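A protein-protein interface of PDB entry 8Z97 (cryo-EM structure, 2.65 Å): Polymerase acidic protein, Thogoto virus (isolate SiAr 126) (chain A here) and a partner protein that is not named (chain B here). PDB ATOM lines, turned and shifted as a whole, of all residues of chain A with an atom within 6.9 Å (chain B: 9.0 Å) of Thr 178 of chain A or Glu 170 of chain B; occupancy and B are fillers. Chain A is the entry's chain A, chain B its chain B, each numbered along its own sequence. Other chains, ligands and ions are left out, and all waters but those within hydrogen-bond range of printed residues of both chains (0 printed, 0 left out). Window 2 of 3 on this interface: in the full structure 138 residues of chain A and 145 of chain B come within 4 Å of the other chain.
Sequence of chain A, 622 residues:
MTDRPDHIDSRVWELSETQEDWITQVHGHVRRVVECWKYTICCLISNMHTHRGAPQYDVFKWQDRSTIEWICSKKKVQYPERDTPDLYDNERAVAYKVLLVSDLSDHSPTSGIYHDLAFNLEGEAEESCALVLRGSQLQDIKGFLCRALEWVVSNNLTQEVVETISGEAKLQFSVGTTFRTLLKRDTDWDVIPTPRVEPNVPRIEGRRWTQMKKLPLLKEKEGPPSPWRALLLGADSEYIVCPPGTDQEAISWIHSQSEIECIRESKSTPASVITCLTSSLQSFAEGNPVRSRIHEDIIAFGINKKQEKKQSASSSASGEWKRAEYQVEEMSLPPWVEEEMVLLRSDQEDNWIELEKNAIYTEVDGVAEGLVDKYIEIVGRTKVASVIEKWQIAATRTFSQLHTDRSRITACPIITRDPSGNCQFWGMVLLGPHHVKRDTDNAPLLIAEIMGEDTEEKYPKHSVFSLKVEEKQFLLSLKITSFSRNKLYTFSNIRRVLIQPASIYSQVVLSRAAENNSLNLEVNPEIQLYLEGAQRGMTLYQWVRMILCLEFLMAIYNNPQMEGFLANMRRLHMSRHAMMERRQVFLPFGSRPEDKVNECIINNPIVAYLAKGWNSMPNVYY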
ATOM      1  N   SER A 174     -12.127 -13.871   6.923  1.00  0.00           N
ATOM      2  CA  SER A 174     -11.828 -14.280   8.285  1.00  0.00           C
ATOM      3  C   SER A 174     -12.650 -13.451   9.256  1.00  0.00           C
ATOM      4  O   SER A 174     -12.880 -12.259   9.029  1.00  0.00           O
ATOM      5  CB  SER A 174     -10.334 -14.130   8.599  1.00  0.00           C
ATOM      6  OG  SER A 174      -9.934 -12.773   8.541  1.00  0.00           O
ATOM      7  N   VAL A 175     -13.093 -14.090  10.333  1.00  0.00           N
ATOM      8  CA  VAL A 175     -13.829 -13.434  11.406  1.00  0.00           C
ATOM      9  C   VAL A 175     -12.945 -13.421  12.643  1.00  0.00           C
ATOM     10  O   VAL A 175     -12.441 -14.469  13.064  1.00  0.00           O
ATOM     11  CB  VAL A 175     -15.166 -14.139  11.689  1.00  0.00           C
ATOM     12  CG1 VAL A 175     -16.022 -13.298  12.616  1.00  0.00           C
ATOM     13  CG2 VAL A 175     -15.902 -14.418  10.390  1.00  0.00           C
ATOM     14  N   GLY A 176     -12.756 -12.241  13.220  1.00  0.00           N
ATOM     15  CA  GLY A 176     -11.901 -12.085  14.375  1.00  0.00           C
ATOM     16  C   GLY A 176     -12.549 -12.601  15.643  1.00  0.00           C
ATOM     17  O   GLY A 176     -13.607 -13.232  15.635  1.00  0.00           O
ATOM     18  N   THR A 177     -11.885 -12.319  16.764  1.00  0.00           N
ATOM     19  CA  THR A 177     -12.360 -12.816  18.050  1.00  0.00           C
ATOM     20  C   THR A 177     -13.494 -11.957  18.599  1.00  0.00           C
ATOM     21  O   THR A 177     -14.543 -12.480  18.985  1.00  0.00           O
ATOM     22  CB  THR A 177     -11.203 -12.877  19.048  1.00  0.00           C
ATOM     23  OG1 THR A 177     -10.124 -13.634  18.485  1.00  0.00           O
ATOM     24  CG2 THR A 177     -11.653 -13.537  20.342  1.00  0.00           C
ATOM     25  N   THR A 178     -13.298 -10.637  18.643  1.00  0.00           N
ATOM     26  CA  THR A 178     -14.315  -9.757  19.213  1.00  0.00           C
ATOM     27  C   THR A 178     -15.601  -9.788  18.397  1.00  0.00           C
ATOM     28  O   THR A 178     -16.703  -9.823  18.960  1.00  0.00           O
ATOM     29  CB  THR A 178     -13.781  -8.328  19.310  1.00  0.00           C
ATOM     30  OG1 THR A 178     -13.464  -7.846  17.999  1.00  0.00           O
ATOM     31  CG2 THR A 178     -12.530  -8.287  20.172  1.00  0.00           C
ATOM     32  N   PHE A 179     -15.480  -9.775  17.068  1.00  0.00           N
ATOM     33  CA  PHE A 179     -16.667  -9.822  16.222  1.00  0.00           C
ATOM     34  C   PHE A 179     -17.410 -11.139  16.394  1.00  0.00           C
ATOM     35  O   PHE A 179     -18.643 -11.171  16.360  1.00  0.00           O
ATOM     36  CB  PHE A 179     -16.280  -9.600  14.760  1.00  0.00           C
ATOM     37  CG  PHE A 179     -17.456  -9.463  13.835  1.00  0.00           C
ATOM     38  CD1 PHE A 179     -18.554  -8.703  14.197  1.00  0.00           C
ATOM     39  CD2 PHE A 179     -17.455 -10.078  12.595  1.00  0.00           C
ATOM     40  CE1 PHE A 179     -19.635  -8.572  13.348  1.00  0.00           C
ATOM     41  CE2 PHE A 179     -18.531  -9.948  11.741  1.00  0.00           C
ATOM     42  CZ  PHE A 179     -19.622  -9.194  12.118  1.00  0.00           C
ATOM     43  N   ARG A 180     -16.677 -12.236  16.588  1.00  0.00           N
ATOM     44  CA  ARG A 180     -17.318 -13.522  16.842  1.00  0.00           C
ATOM     45  C   ARG A 180     -18.113 -13.498  18.144  1.00  0.00           C
ATOM     46  O   ARG A 180     -19.236 -14.013  18.206  1.00  0.00           O
ATOM     47  CB  ARG A 180     -16.264 -14.627  16.873  1.00  0.00           C
ATOM     48  CG  ARG A 180     -16.824 -16.033  16.904  1.00  0.00           C
ATOM     49  CD  ARG A 180     -15.706 -17.061  16.865  1.00  0.00           C
ATOM     50  NE  ARG A 180     -14.829 -16.864  15.717  1.00  0.00           N
ATOM     51  CZ  ARG A 180     -14.950 -17.505  14.563  1.00  0.00           C
ATOM     52  NH1 ARG A 180     -15.896 -18.408  14.370  1.00  0.00           N
ATOM     53  NH2 ARG A 180     -14.098 -17.234  13.579  1.00  0.00           N
ATOM     54  N   THR A 181     -17.544 -12.903  19.196  1.00  0.00           N
ATOM     55  CA  THR A 181     -18.260 -12.798  20.464  1.00  0.00           C
ATOM     56  C   THR A 181     -19.500 -11.923  20.329  1.00  0.00           C
ATOM     57  O   THR A 181     -20.550 -12.231  20.904  1.00  0.00           O
ATOM     58  CB  THR A 181     -17.340 -12.249  21.554  1.00  0.00           C
ATOM     59  OG1 THR A 181     -16.965 -10.902  21.234  1.00  0.00           O
ATOM     60  CG2 THR A 181     -16.092 -13.108  21.686  1.00  0.00           C
ATOM     61  N   LEU A 182     -19.395 -10.818  19.586  1.00  0.00           N
ATOM     62  CA  LEU A 182     -20.570  -9.986  19.345  1.00  0.00           C
ATOM     63  C   LEU A 182     -21.636 -10.751  18.574  1.00  0.00           C
ATOM     64  O   LEU A 182     -22.831 -10.645  18.873  1.00  0.00           O
ATOM     65  CB  LEU A 182     -20.175  -8.718  18.588  1.00  0.00           C
ATOM     66  CG  LEU A 182     -19.899  -7.456  19.408  1.00  0.00           C
ATOM     67  CD1 LEU A 182     -18.807  -7.696  20.435  1.00  0.00           C
ATOM     68  CD2 LEU A 182     -19.530  -6.308  18.489  1.00  0.00           C
ATOM     69  N   LEU A 183     -21.218 -11.528  17.575  1.00  0.00           N
ATOM     70  CA  LEU A 183     -22.160 -12.280  16.756  1.00  0.00           C
ATOM     71  C   LEU A 183     -22.881 -13.350  17.563  1.00  0.00           C
ATOM     72  O   LEU A 183     -24.088 -13.554  17.393  1.00  0.00           O
ATOM     73  CB  LEU A 183     -21.420 -12.908  15.579  1.00  0.00           C
ATOM     74  CG  LEU A 183     -21.063 -11.998  14.407  1.00  0.00           C
ATOM     75  CD1 LEU A 183     -19.997 -12.659  13.563  1.00  0.00           C
ATOM     76  CD2 LEU A 183     -22.294 -11.701  13.579  1.00  0.00           C
ATOM     77  N   ARG A 185     -23.953 -13.482  20.489  1.00  0.00           N
ATOM     78  CA  ARG A 185     -24.667 -13.019  21.673  1.00  0.00           C
ATOM     79  C   ARG A 185     -26.101 -13.532  21.708  1.00  0.00           C
ATOM     80  O   ARG A 185     -26.594 -13.935  22.766  1.00  0.00           O
ATOM     81  CB  ARG A 185     -24.646 -11.494  21.731  1.00  0.00           C
ATOM     82  CG  ARG A 185     -23.315 -10.915  22.160  1.00  0.00           C
ATOM     83  CD  ARG A 185     -23.392  -9.408  22.298  1.00  0.00           C
ATOM     84  NE  ARG A 185     -22.143  -8.849  22.800  1.00  0.00           N
ATOM     85  CZ  ARG A 185     -21.904  -7.552  22.929  1.00  0.00           C
ATOM     86  NH1 ARG A 185     -22.811  -6.647  22.602  1.00  0.00           N
ATOM     87  NH2 ARG A 185     -20.725  -7.154  23.395  1.00  0.00           N
ATOM     88  N   LEU B 150      -9.860   1.803   8.075  1.00  0.00           N
ATOM     89  CA  LEU B 150      -8.949   0.682   7.912  1.00  0.00           C
ATOM     90  C   LEU B 150      -7.589   1.087   7.360  1.00  0.00           C
ATOM     91  O   LEU B 150      -6.683   0.249   7.323  1.00  0.00           O
ATOM     92  CB  LEU B 150      -9.576  -0.374   6.998  1.00  0.00           C
ATOM     93  CG  LEU B 150     -10.697  -1.202   7.624  1.00  0.00           C
ATOM     94  CD1 LEU B 150     -11.172  -2.260   6.654  1.00  0.00           C
ATOM     95  CD2 LEU B 150     -10.231  -1.836   8.923  1.00  0.00           C
ATOM     96  N   GLN B 163     -15.041  -8.365   4.018  1.00  0.00           N
ATOM     97  CA  GLN B 163     -13.861  -8.464   4.867  1.00  0.00           C
ATOM     98  C   GLN B 163     -13.556  -7.131   5.537  1.00  0.00           C
ATOM     99  O   GLN B 163     -13.131  -7.094   6.695  1.00  0.00           O
ATOM    100  CB  GLN B 163     -12.663  -8.943   4.050  1.00  0.00           C
ATOM    101  CG  GLN B 163     -11.388  -9.082   4.857  1.00  0.00           C
ATOM    102  CD  GLN B 163     -11.524 -10.089   5.979  1.00  0.00           C
ATOM    103  OE1 GLN B 163     -11.807 -11.262   5.743  1.00  0.00           O
ATOM    104  NE2 GLN B 163     -11.325  -9.634   7.209  1.00  0.00           N
ATOM    105  N   ALA B 164     -13.767  -6.025   4.822  1.00  0.00           N
ATOM    106  CA  ALA B 164     -13.582  -4.709   5.422  1.00  0.00           C
ATOM    107  C   ALA B 164     -14.566  -4.480   6.560  1.00  0.00           C
ATOM    108  O   ALA B 164     -14.207  -3.907   7.594  1.00  0.00           O
ATOM    109  CB  ALA B 164     -13.728  -3.623   4.359  1.00  0.00           C
ATOM    110  N   ILE B 165     -15.818  -4.906   6.381  1.00  0.00           N
ATOM    111  CA  ILE B 165     -16.800  -4.793   7.460  1.00  0.00           C
ATOM    112  C   ILE B 165     -16.353  -5.609   8.669  1.00  0.00           C
ATOM    113  O   ILE B 165     -16.378  -5.135   9.814  1.00  0.00           O
ATOM    114  CB  ILE B 165     -18.191  -5.231   6.972  1.00  0.00           C
ATOM    115  CG1 ILE B 165     -18.663  -4.349   5.817  1.00  0.00           C
ATOM    116  CG2 ILE B 165     -19.191  -5.181   8.111  1.00  0.00           C
ATOM    117  CD1 ILE B 165     -18.846  -2.906   6.193  1.00  0.00           C
ATOM    118  N   ALA B 166     -15.923  -6.849   8.426  1.00  0.00           N
ATOM    119  CA  ALA B 166     -15.488  -7.710   9.521  1.00  0.00           C
ATOM    120  C   ALA B 166     -14.271  -7.130  10.231  1.00  0.00           C
ATOM    121  O   ALA B 166     -14.131  -7.268  11.452  1.00  0.00           O
ATOM    122  CB  ALA B 166     -15.185  -9.113   8.997  1.00  0.00           C
ATOM    123  N   ASP B 167     -13.379  -6.477   9.484  1.00  0.00           N
ATOM    124  CA  ASP B 167     -12.179  -5.908  10.086  1.00  0.00           C
ATOM    125  C   ASP B 167     -12.497  -4.653  10.888  1.00  0.00           C
ATOM    126  O   ASP B 167     -11.957  -4.461  11.984  1.00  0.00           O
ATOM    127  CB  ASP B 167     -11.145  -5.602   9.005  1.00  0.00           C
ATOM    128  CG  ASP B 167     -10.538  -6.854   8.410  1.00  0.00           C
ATOM    129  OD1 ASP B 167     -10.806  -7.954   8.937  1.00  0.00           O
ATOM    130  OD2 ASP B 167      -9.792  -6.740   7.415  1.00  0.00           O
ATOM    131  N   VAL B 168     -13.357  -3.779  10.360  1.00  0.00           N
ATOM    132  CA  VAL B 168     -13.703  -2.569  11.097  1.00  0.00           C
ATOM    133  C   VAL B 168     -14.513  -2.912  12.338  1.00  0.00           C
ATOM    134  O   VAL B 168     -14.496  -2.153  13.315  1.00  0.00           O
ATOM    135  CB  VAL B 168     -14.464  -1.566  10.207  1.00  0.00           C
ATOM    136  CG1 VAL B 168     -15.821  -2.110   9.815  1.00  0.00           C
ATOM    137  CG2 VAL B 168     -14.590  -0.213  10.892  1.00  0.00           C
ATOM    138  N   MET B 169     -15.215  -4.049  12.338  1.00  0.00           N
ATOM    139  CA  MET B 169     -15.890  -4.481  13.555  1.00  0.00           C
ATOM    140  C   MET B 169     -14.912  -4.798  14.681  1.00  0.00           C
ATOM    141  O   MET B 169     -15.317  -4.822  15.847  1.00  0.00           O
ATOM    142  CB  MET B 169     -16.763  -5.703  13.267  1.00  0.00           C
ATOM    143  CG  MET B 169     -18.130  -5.361  12.706  1.00  0.00           C
ATOM    144  SD  MET B 169     -18.909  -3.986  13.569  1.00  0.00           S
ATOM    145  CE  MET B 169     -19.495  -4.805  15.048  1.00  0.00           C
ATOM    146  N   GLU B 170     -13.640  -5.044  14.359  1.00  0.00           N
ATOM    147  CA  GLU B 170     -12.646  -5.354  15.381  1.00  0.00           C
ATOM    148  C   GLU B 170     -12.162  -4.116  16.125  1.00  0.00           C
ATOM    149  O   GLU B 170     -11.813  -4.211  17.307  1.00  0.00           O
ATOM    150  CB  GLU B 170     -11.453  -6.073  14.750  1.00  0.00           C
ATOM    151  CG  GLU B 170     -11.794  -7.430  14.175  1.00  0.00           C
ATOM    152  CD  GLU B 170     -12.141  -8.437  15.248  1.00  0.00           C
ATOM    153  OE1 GLU B 170     -11.502  -8.410  16.321  1.00  0.00           O
ATOM    154  OE2 GLU B 170     -13.063  -9.247  15.025  1.00  0.00           O
ATOM    155  N   LEU B 171     -12.121  -2.963  15.461  1.00  0.00           N
ATOM    156  CA  LEU B 171     -11.563  -1.765  16.073  1.00  0.00           C
ATOM    157  C   LEU B 171     -12.405  -1.310  17.259  1.00  0.00           C
ATOM    158  O   LEU B 171     -13.637  -1.379  17.233  1.00  0.00           O
ATOM    159  CB  LEU B 171     -11.461  -0.640  15.045  1.00  0.00           C
ATOM    160  CG  LEU B 171     -10.942  -1.032  13.661  1.00  0.00           C
ATOM    161  CD1 LEU B 171     -11.004   0.153  12.713  1.00  0.00           C
ATOM    162  CD2 LEU B 171      -9.528  -1.579  13.751  1.00  0.00           C
ATOM    163  N   ASP B 172     -11.724  -0.848  18.311  1.00  0.00           N
ATOM    164  CA  ASP B 172     -12.423  -0.379  19.503  1.00  0.00           C
ATOM    165  C   ASP B 172     -13.221   0.888  19.220  1.00  0.00           C
ATOM    166  O   ASP B 172     -14.368   1.017  19.663  1.00  0.00           O
ATOM    167  CB  ASP B 172     -11.421  -0.134  20.632  1.00  0.00           C
ATOM    168  CG  ASP B 172     -10.799  -1.415  21.148  1.00  0.00           C
ATOM    169  OD1 ASP B 172     -11.465  -2.468  21.087  1.00  0.00           O
ATOM    170  OD2 ASP B 172      -9.642  -1.369  21.614  1.00  0.00           O
ATOM    171  N   GLU B 173     -12.633   1.833  18.490  1.00  0.00           N
ATOM    172  CA  GLU B 173     -13.255   3.122  18.229  1.00  0.00           C
ATOM    173  C   GLU B 173     -13.048   3.482  16.766  1.00  0.00           C
ATOM    174  O   GLU B 173     -11.980   3.228  16.204  1.00  0.00           O
ATOM    175  CB  GLU B 173     -12.667   4.206  19.148  1.00  0.00           C
ATOM    176  CG  GLU B 173     -13.395   5.544  19.134  1.00  0.00           C
ATOM    177  CD  GLU B 173     -12.964   6.445  17.993  1.00  0.00           C
ATOM    178  OE1 GLU B 173     -11.803   6.329  17.549  1.00  0.00           O
ATOM    179  OE2 GLU B 173     -13.785   7.273  17.545  1.00  0.00           O
ATOM    180  N   THR B 174     -14.073   4.072  16.154  1.00  0.00           N
ATOM    181  CA  THR B 174     -14.033   4.440  14.748  1.00  0.00           C
ATOM    182  C   THR B 174     -14.565   5.853  14.561  1.00  0.00           C
ATOM    183  O   THR B 174     -15.358   6.349  15.366  1.00  0.00           O
ATOM    184  CB  THR B 174     -14.841   3.462  13.882  1.00  0.00           C
ATOM    185  OG1 THR B 174     -16.087   3.167  14.523  1.00  0.00           O
ATOM    186  CG2 THR B 174     -14.068   2.172  13.672  1.00  0.00           C
ATOM    187  N   SER B 215     -18.149   3.384  18.572  1.00  0.00           N
ATOM    188  CA  SER B 215     -17.449   2.383  19.359  1.00  0.00           C
ATOM    189  C   SER B 215     -17.818   1.021  18.789  1.00  0.00           C
ATOM    190  O   SER B 215     -18.634   0.918  17.870  1.00  0.00           O
ATOM    191  CB  SER B 215     -17.805   2.489  20.846  1.00  0.00           C
ATOM    192  OG  SER B 215     -17.782   3.837  21.278  1.00  0.00           O
ATOM    193  N   ARG B 216     -17.211  -0.038  19.328  1.00  0.00           N
ATOM    194  CA  ARG B 216     -17.603  -1.374  18.895  1.00  0.00           C
ATOM    195  C   ARG B 216     -19.067  -1.639  19.215  1.00  0.00           C
ATOM    196  O   ARG B 216     -19.803  -2.182  18.383  1.00  0.00           O
ATOM    197  CB  ARG B 216     -16.715  -2.437  19.539  1.00  0.00           C
ATOM    198  CG  ARG B 216     -16.732  -3.758  18.784  1.00  0.00           C
ATOM    199  CD  ARG B 216     -15.912  -4.829  19.479  1.00  0.00           C
ATOM    200  NE  ARG B 216     -14.495  -4.736  19.156  1.00  0.00           N
ATOM    201  CZ  ARG B 216     -13.552  -4.392  20.023  1.00  0.00           C
ATOM    202  NH1 ARG B 216     -13.844  -4.093  21.278  1.00  0.00           N
ATOM    203  NH2 ARG B 216     -12.286  -4.346  19.620  1.00  0.00           N
ATOM    204  N   GLU B 217     -19.512  -1.246  20.409  1.00  0.00           N
ATOM    205  CA  GLU B 217     -20.914  -1.424  20.769  1.00  0.00           C
ATOM    206  C   GLU B 217     -21.824  -0.551  19.913  1.00  0.00           C
ATOM    207  O   GLU B 217     -22.865  -1.015  19.435  1.00  0.00           O
ATOM    208  CB  GLU B 217     -21.115  -1.117  22.252  1.00  0.00           C
ATOM    209  CG  GLU B 217     -20.890  -2.311  23.157  1.00  0.00           C
ATOM    210  CD  GLU B 217     -21.976  -3.357  23.019  1.00  0.00           C
ATOM    211  OE1 GLU B 217     -23.169  -2.987  23.035  1.00  0.00           O
ATOM    212  OE2 GLU B 217     -21.637  -4.551  22.891  1.00  0.00           O
ATOM    213  N   LEU B 219     -21.188   0.778  16.876  1.00  0.00           N
ATOM    214  CA  LEU B 219     -21.179   0.299  15.498  1.00  0.00           C
ATOM    215  C   LEU B 219     -21.960  -1.003  15.367  1.00  0.00           C
ATOM    216  O   LEU B 219     -22.658  -1.217  14.370  1.00  0.00           O
ATOM    217  CB  LEU B 219     -19.743   0.121  15.010  1.00  0.00           C
ATOM    218  CG  LEU B 219     -19.571  -0.214  13.528  1.00  0.00           C
ATOM    219  CD1 LEU B 219     -20.139   0.898  12.665  1.00  0.00           C
ATOM    220  CD2 LEU B 219     -18.109  -0.452  13.201  1.00  0.00           C
ATOM    221  N   TRP B 220     -21.854  -1.883  16.364  1.00  0.00           N
ATOM    222  CA  TRP B 220     -22.650  -3.104  16.364  1.00  0.00           C
ATOM    223  C   TRP B 220     -24.138  -2.787  16.382  1.00  0.00           C
ATOM    224  O   TRP B 220     -24.916  -3.379  15.625  1.00  0.00           O
ATOM    225  CB  TRP B 220     -22.267  -3.969  17.565  1.00  0.00           C
ATOM    226  CG  TRP B 220     -23.035  -5.252  17.689  1.00  0.00           C
ATOM    227  CD1 TRP B 220     -23.702  -5.696  18.790  1.00  0.00           C
ATOM    228  CD2 TRP B 220     -23.191  -6.267  16.689  1.00  0.00           C
ATOM    229  NE1 TRP B 220     -24.277  -6.916  18.538  1.00  0.00           N
ATOM    230  CE2 TRP B 220     -23.976  -7.290  17.255  1.00  0.00           C
ATOM    231  CE3 TRP B 220     -22.749  -6.408  15.371  1.00  0.00           C
ATOM    232  CZ2 TRP B 220     -24.330  -8.436  16.547  1.00  0.00           C
ATOM    233  CZ3 TRP B 220     -23.100  -7.547  14.673  1.00  0.00           C
ATOM    234  CH2 TRP B 220     -23.882  -8.546  15.262  1.00  0.00           C
ATOM    235  N   MET B 223     -25.196  -1.542  12.991  1.00  0.00           N
ATOM    236  CA  MET B 223     -25.269  -2.606  11.993  1.00  0.00           C
ATOM    237  C   MET B 223     -26.496  -3.483  12.202  1.00  0.00           C
ATOM    238  O   MET B 223     -27.139  -3.903  11.233  1.00  0.00           O
ATOM    239  CB  MET B 223     -23.996  -3.449  12.027  1.00  0.00           C
ATOM    240  CG  MET B 223     -24.049  -4.667  11.120  1.00  0.00           C
ATOM    241  SD  MET B 223     -22.864  -5.940  11.579  1.00  0.00           S
ATOM    242  CE  MET B 223     -21.342  -5.169  11.045  1.00  0.00           C
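OE2 of Glu 170 of chain B is in hydrogen-bond range of N of Phe 179 of chain A (3.2 Å).
The guanidinium group of Arg 216 of chain B lies within hydrogen-bond range of the side-chain hydroxyl of Thr 178 of chain A.
OG1 of Thr 178 of chain A lies within hydrogen-bond range of OE1 of Glu 170 of chain B.
The backbone NH of Ser 174 of chain A sits at hydrogen-bond distance from the side-chain amide oxygen of Gln 163 of chain B (2.9 Å).
OE2 of Glu 217 of chain B is in salt-bridge range of NH1 of Arg 185 of chain A (2.4 Å).
The side-chain carboxylate (OD1) of Asp 172 of chain B lies within salt-bridge range of the guanidinium group (NH2) of Arg 216 of chain B, 2.5 Å away.
NE2 of Gln 163 of chain B lies within hydrogen-bond range of OD1 of Asp 167 of chain B.
The backbone carbonyl oxygen of Glu 170 of chain B lies close to the guanidinium group of Arg 216 of chain B, 3.3 Å away.
O of Met 169 of chain B lies within hydrogen-bond range of NE of Arg 216 of chain B (3.4 Å).
The side-chain hydroxyl of Thr 181 of chain A lies within hydrogen-bond range of the backbone carbonyl oxygen of Thr 178 of chain A, 2.5 Å away.
Of the printed residues of chain B, Gly 176 of chain A touches Glu 170 (3.1 Å).
Thr 178 of chain A touches just these residues of chain B: Glu 170 (2.6 Å) and Arg 216 (3.5 Å).
Printed residues of chain B within 4 Å of Phe 179 of chain A: Met 169, Glu 170 and Trp 220.
Of chain A, only Gly 176, Thr 177, Thr 178 and Phe 179 come within 4 Å of Glu 170 of chain B.
Printed residues of chain A within 4 Å of Arg 216 of chain B: Thr 178 and Leu 182.
Printed residues of chain A within 4 Å of Glu 217 of chain B: Arg 185 (2.4 Å).
The nearest residue of chain B that does not touch Thr 178 of chain A is Met 169 of chain B (4.1 Å).
Among the printed residues, merely in contact across the chains: Ser 174 of chain A with Ala 166 of chain B (3.9 Å), Gly 176 of chain A with Glu 170 of chain B (3.1 Å), Thr 177 of chain A with Glu 170 of chain B (3.7 Å), Phe 179 of chain A with Met 169 of chain B (3.6 Å), Phe 179 of chain A with Trp 220 of chain B (3.8 Å), Leu 182 of chain A with Met 169 of chain B (3.8 Å), Leu 182 of chain A with Arg 216 of chain B (3.8 Å), Leu 182 of chain A with Trp 220 of chain B (3.5 Å) and Leu 183 of chain A with Trp 220 of chain B (3.9 Å).
Printed residues of chain B that touch a printed residue of chain A: Gln 163, Ala 166, Met 169, Glu 170, Arg 216, Glu 217 and Trp 220.
Hydrophobic or aromatic side chains of chain B that line the printed part of chain A: Ala 166, Met 169 and Trp 220.
Along chain B the printed residues that touch a printed residue of chain A span positions 163 to 220.
Of the 11 printed residues of chain A, 8 touch a printed residue of chain B.
Hydrophobic or aromatic side chains of chain A that line the printed part of chain B: Phe 179, Leu 182 and Leu 183.
Among the printed residues, 14 pairs touch across the chains.
Among the printed residues, Asp or Glu carboxylates within 4 Å of a Lys or Arg side-chain nitrogen of the other chain: Arg 185 of chain A with Glu 217 of chain B.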
